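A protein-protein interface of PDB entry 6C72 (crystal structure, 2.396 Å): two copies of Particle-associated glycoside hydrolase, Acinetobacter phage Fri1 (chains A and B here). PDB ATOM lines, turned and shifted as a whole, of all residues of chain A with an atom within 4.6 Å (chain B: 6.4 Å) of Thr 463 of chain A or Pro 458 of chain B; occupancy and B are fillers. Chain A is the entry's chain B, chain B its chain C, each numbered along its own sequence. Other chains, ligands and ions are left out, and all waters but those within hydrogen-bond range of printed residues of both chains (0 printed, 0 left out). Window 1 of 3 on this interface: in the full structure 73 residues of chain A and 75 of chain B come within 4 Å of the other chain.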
ATOM      1  N   ASP A 420       0.960  22.336   0.482  1.00  0.00           N
ATOM      2  CA  ASP A 420       0.988  21.463  -0.682  1.00  0.00           C
ATOM      3  C   ASP A 420       0.745  20.014  -0.308  1.00  0.00           C
ATOM      4  O   ASP A 420       0.833  19.138  -1.177  1.00  0.00           O
ATOM      5  CB  ASP A 420       2.323  21.609  -1.426  1.00  0.00           C
ATOM      6  CG  ASP A 420       2.536  23.023  -1.953  1.00  0.00           C
ATOM      7  OD1 ASP A 420       1.576  23.580  -2.520  1.00  0.00           O
ATOM      8  OD2 ASP A 420       3.643  23.589  -1.764  1.00  0.00           O
ATOM      9  N   ARG A 461      -4.496  26.029   0.829  1.00  0.00           N
ATOM     10  CA  ARG A 461      -3.231  26.609   1.267  1.00  0.00           C
ATOM     11  C   ARG A 461      -2.116  26.269   0.287  1.00  0.00           C
ATOM     12  O   ARG A 461      -0.937  26.383   0.626  1.00  0.00           O
ATOM     13  CB  ARG A 461      -2.868  26.137   2.686  1.00  0.00           C
ATOM     14  CG  ARG A 461      -3.971  26.402   3.722  1.00  0.00           C
ATOM     15  CD  ARG A 461      -3.493  26.222   5.167  1.00  0.00           C
ATOM     16  NE  ARG A 461      -4.497  26.696   6.116  1.00  0.00           N
ATOM     17  CZ  ARG A 461      -5.138  25.937   7.014  1.00  0.00           C
ATOM     18  NH1 ARG A 461      -4.882  24.647   7.125  1.00  0.00           N
ATOM     19  NH2 ARG A 461      -6.040  26.482   7.826  1.00  0.00           N
ATOM     20  N   ARG A 462      -2.468  25.865  -0.923  1.00  0.00           N
ATOM     21  CA  ARG A 462      -1.463  25.421  -1.870  1.00  0.00           C
ATOM     22  C   ARG A 462      -0.665  26.595  -2.425  1.00  0.00           C
ATOM     23  O   ARG A 462      -1.153  27.726  -2.523  1.00  0.00           O
ATOM     24  CB  ARG A 462      -2.121  24.644  -3.008  1.00  0.00           C
ATOM     25  CG  ARG A 462      -2.694  23.304  -2.589  1.00  0.00           C
ATOM     26  CD  ARG A 462      -3.585  22.773  -3.674  1.00  0.00           C
ATOM     27  NE  ARG A 462      -4.734  23.640  -3.892  1.00  0.00           N
ATOM     28  CZ  ARG A 462      -5.393  23.719  -5.042  1.00  0.00           C
ATOM     29  NH1 ARG A 462      -5.001  22.989  -6.068  1.00  0.00           N
ATOM     30  NH2 ARG A 462      -6.442  24.523  -5.167  1.00  0.00           N
ATOM     31  N   THR A 463       0.586  26.308  -2.784  1.00  0.00           N
ATOM     32  CA  THR A 463       1.450  27.342  -3.332  1.00  0.00           C
ATOM     33  C   THR A 463       0.960  27.824  -4.691  1.00  0.00           C
ATOM     34  O   THR A 463       0.928  29.033  -4.943  1.00  0.00           O
ATOM     35  CB  THR A 463       2.875  26.812  -3.435  1.00  0.00           C
ATOM     36  OG1 THR A 463       3.341  26.458  -2.128  1.00  0.00           O
ATOM     37  CG2 THR A 463       3.789  27.857  -4.017  1.00  0.00           C
ATOM     38  N   ILE A 464       0.496  26.907  -5.545  1.00  0.00           N
ATOM     39  CA  ILE A 464       0.106  27.271  -6.907  1.00  0.00           C
ATOM     40  C   ILE A 464      -0.991  28.321  -6.895  1.00  0.00           C
ATOM     41  O   ILE A 464      -1.065  29.156  -7.802  1.00  0.00           O
ATOM     42  CB  ILE A 464      -0.315  26.018  -7.721  1.00  0.00           C
ATOM     43  CG1 ILE A 464      -0.658  26.377  -9.169  1.00  0.00           C
ATOM     44  CG2 ILE A 464      -1.551  25.373  -7.141  1.00  0.00           C
ATOM     45  CD1 ILE A 464       0.507  26.865  -9.991  1.00  0.00           C
ATOM     46  N   THR A 465      -1.839  28.329  -5.872  1.00  0.00           N
ATOM     47  CA  THR A 465      -2.940  29.285  -5.803  1.00  0.00           C
ATOM     48  C   THR A 465      -2.689  30.438  -4.827  1.00  0.00           C
ATOM     49  O   THR A 465      -3.629  31.167  -4.510  1.00  0.00           O
ATOM     50  CB  THR A 465      -4.237  28.574  -5.414  1.00  0.00           C
ATOM     51  OG1 THR A 465      -4.003  27.808  -4.226  1.00  0.00           O
ATOM     52  CG2 THR A 465      -4.737  27.678  -6.553  1.00  0.00           C
ATOM     53  N   GLN A 466      -1.462  30.613  -4.336  1.00  0.00           N
ATOM     54  CA  GLN A 466      -1.236  31.626  -3.305  1.00  0.00           C
ATOM     55  C   GLN A 466      -1.519  33.040  -3.815  1.00  0.00           C
ATOM     56  O   GLN A 466      -1.913  33.912  -3.033  1.00  0.00           O
ATOM     57  CB  GLN A 466       0.195  31.529  -2.774  1.00  0.00           C
ATOM     58  CG  GLN A 466       1.257  31.995  -3.760  1.00  0.00           C
ATOM     59  CD  GLN A 466       2.665  31.620  -3.316  1.00  0.00           C
ATOM     60  OE1 GLN A 466       2.856  31.083  -2.222  1.00  0.00           O
ATOM     61  NE2 GLN A 466       3.655  31.903  -4.161  1.00  0.00           N
ATOM     62  N   PHE B 444       3.650  27.331 -13.069  1.00  0.00           N
ATOM     63  CA  PHE B 444       4.726  26.879 -12.196  1.00  0.00           C
ATOM     64  C   PHE B 444       4.178  26.713 -10.783  1.00  0.00           C
ATOM     65  O   PHE B 444       3.557  27.637 -10.239  1.00  0.00           O
ATOM     66  CB  PHE B 444       5.908  27.871 -12.177  1.00  0.00           C
ATOM     67  CG  PHE B 444       6.742  27.866 -13.436  1.00  0.00           C
ATOM     68  CD1 PHE B 444       6.350  28.609 -14.554  1.00  0.00           C
ATOM     69  CD2 PHE B 444       7.922  27.132 -13.501  1.00  0.00           C
ATOM     70  CE1 PHE B 444       7.109  28.605 -15.719  1.00  0.00           C
ATOM     71  CE2 PHE B 444       8.690  27.118 -14.669  1.00  0.00           C
ATOM     72  CZ  PHE B 444       8.280  27.865 -15.776  1.00  0.00           C
ATOM     73  N   GLY B 445       4.387  25.537 -10.200  1.00  0.00           N
ATOM     74  CA  GLY B 445       4.208  25.333  -8.772  1.00  0.00           C
ATOM     75  C   GLY B 445       5.518  25.550  -8.047  1.00  0.00           C
ATOM     76  O   GLY B 445       6.401  26.270  -8.523  1.00  0.00           O
ATOM     77  N   VAL B 446       5.669  24.899  -6.894  1.00  0.00           N
ATOM     78  CA  VAL B 446       6.962  24.902  -6.221  1.00  0.00           C
ATOM     79  C   VAL B 446       7.957  24.133  -7.078  1.00  0.00           C
ATOM     80  O   VAL B 446       7.657  23.048  -7.585  1.00  0.00           O
ATOM     81  CB  VAL B 446       6.858  24.273  -4.822  1.00  0.00           C
ATOM     82  CG1 VAL B 446       8.239  24.145  -4.188  1.00  0.00           C
ATOM     83  CG2 VAL B 446       5.966  25.068  -3.926  1.00  0.00           C
ATOM     84  N   ASN B 447       9.146  24.693  -7.254  1.00  0.00           N
ATOM     85  CA  ASN B 447      10.237  23.975  -7.885  1.00  0.00           C
ATOM     86  C   ASN B 447      11.513  24.299  -7.125  1.00  0.00           C
ATOM     87  O   ASN B 447      11.595  25.302  -6.406  1.00  0.00           O
ATOM     88  CB  ASN B 447      10.396  24.337  -9.366  1.00  0.00           C
ATOM     89  CG  ASN B 447       9.220  23.879 -10.215  1.00  0.00           C
ATOM     90  OD1 ASN B 447       9.126  22.697 -10.591  1.00  0.00           O
ATOM     91  ND2 ASN B 447       8.320  24.814 -10.534  1.00  0.00           N
ATOM     92  N   ILE B 456      12.214  30.815 -11.050  1.00  0.00           N
ATOM     93  CA  ILE B 456      10.891  31.174 -11.545  1.00  0.00           C
ATOM     94  C   ILE B 456       9.937  31.116 -10.361  1.00  0.00           C
ATOM     95  O   ILE B 456       9.817  30.065  -9.715  1.00  0.00           O
ATOM     96  CB  ILE B 456      10.429  30.238 -12.672  1.00  0.00           C
ATOM     97  CG1 ILE B 456      11.478  30.185 -13.780  1.00  0.00           C
ATOM     98  CG2 ILE B 456       9.085  30.673 -13.222  1.00  0.00           C
ATOM     99  CD1 ILE B 456      11.633  31.477 -14.503  1.00  0.00           C
ATOM    100  N   GLN B 457       9.288  32.233 -10.053  1.00  0.00           N
ATOM    101  CA  GLN B 457       8.297  32.229  -8.992  1.00  0.00           C
ATOM    102  C   GLN B 457       7.086  31.386  -9.389  1.00  0.00           C
ATOM    103  O   GLN B 457       6.699  31.354 -10.560  1.00  0.00           O
ATOM    104  CB  GLN B 457       7.808  33.638  -8.665  1.00  0.00           C
ATOM    105  CG  GLN B 457       8.868  34.612  -8.216  1.00  0.00           C
ATOM    106  CD  GLN B 457       9.680  34.107  -7.048  1.00  0.00           C
ATOM    107  OE1 GLN B 457       9.174  33.371  -6.178  1.00  0.00           O
ATOM    108  NE2 GLN B 457      10.955  34.531  -6.993  1.00  0.00           N
ATOM    109  N   PRO B 458       6.454  30.719  -8.422  1.00  0.00           N
ATOM    110  CA  PRO B 458       5.190  30.038  -8.712  1.00  0.00           C
ATOM    111  C   PRO B 458       4.181  31.030  -9.251  1.00  0.00           C
ATOM    112  O   PRO B 458       4.119  32.179  -8.810  1.00  0.00           O
ATOM    113  CB  PRO B 458       4.764  29.481  -7.348  1.00  0.00           C
ATOM    114  CG  PRO B 458       6.047  29.369  -6.565  1.00  0.00           C
ATOM    115  CD  PRO B 458       6.879  30.532  -7.021  1.00  0.00           C
ATOM    116  N   VAL B 459       3.422  30.598 -10.249  1.00  0.00           N
ATOM    117  CA  VAL B 459       2.431  31.455 -10.884  1.00  0.00           C
ATOM    118  C   VAL B 459       1.378  30.547 -11.503  1.00  0.00           C
ATOM    119  O   VAL B 459       1.715  29.530 -12.114  1.00  0.00           O
ATOM    120  CB  VAL B 459       3.070  32.388 -11.936  1.00  0.00           C
ATOM    121  CG1 VAL B 459       3.863  31.596 -12.997  1.00  0.00           C
ATOM    122  CG2 VAL B 459       2.011  33.298 -12.585  1.00  0.00           C
ATOM    123  N   ASP B 460       0.104  30.867 -11.314  1.00  0.00           N
ATOM    124  CA  ASP B 460      -0.971  30.057 -11.869  1.00  0.00           C
ATOM    125  C   ASP B 460      -1.428  30.657 -13.191  1.00  0.00           C
ATOM    126  O   ASP B 460      -1.846  31.816 -13.240  1.00  0.00           O
ATOM    127  CB  ASP B 460      -2.148  29.939 -10.899  1.00  0.00           C
ATOM    128  CG  ASP B 460      -3.197  28.919 -11.369  1.00  0.00           C
ATOM    129  OD1 ASP B 460      -2.902  28.153 -12.316  1.00  0.00           O
ATOM    130  OD2 ASP B 460      -4.302  28.879 -10.783  1.00  0.00           O
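The side-chain carboxylate of Asp 420 of chain A sits at hydrogen-bond distance from the side-chain hydroxyl of Thr 463 of chain A, at 2.9 Å.
The backbone NH (N) of Val 459 of chain B lies within hydrogen-bond range of the backbone carbonyl oxygen (O) of Phe 444 of chain B, at 3.0 Å.
Among the printed residues, merely in contact across the chains: Ile 464 of chain A with Phe 444 of chain B, Ile 464 of chain A with Asp 460 of chain B, Thr 463 of chain A with Val 446 of chain B, Asp 420 of chain A with Val 446 of chain B, Ile 464 of chain A with Val 459 of chain B and Thr 463 of chain A with Pro 458 of chain B.
Arg 461 of chain A touches none of the printed residues of chain B.
Thr 463 of chain A touches just these residues of chain B: Val 446 (3.5 Å) and Pro 458 (3.7 Å).
Printed residues of chain A within 4 Å of Phe 444 of chain B: Ile 464 (3.2 Å).
Of the printed residues of chain A, Val 446 of chain B touches Asp 420 (3.5 Å) and Thr 463 (3.5 Å).
Pro 458 of chain B touches just one residue of chain A: Thr 463.
Printed residues of chain A within 4 Å of Val 459 of chain B: Ile 464.
Of the printed residues of chain A, Asp 460 of chain B touches Ile 464 (3.4 Å).
The nearest residue of chain B that does not touch Thr 463 of chain A is Gly 445 of chain B (5.0 Å).
The nearest residue of chain A that does not touch Pro 458 of chain B is Gln 466 of chain A (4.2 Å).
The nearest printed residue of chain A that does not touch Val 459 of chain B is Thr 463 of chain A (6.1 Å).
Printed residues of chain A that touch a printed residue of chain B: Asp 420, Thr 463 and Ile 464.
Hydrophobic or aromatic side chains of chain A within 4 Å of the printed part of chain B: Ile 464.
Of the 9 printed residues of chain B, 5 touch a printed residue of chain A.
Hydrophobic or aromatic side chains of chain B within 4 Å of the printed part of chain A: Val 446 and Pro 458.
Among the printed residues, 6 pairs touch across the chains.
No position is printed for both chains.
Of the 6 pairs that touch across the chains among the printed residues, none has its exchanged pair printed and touching as well.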
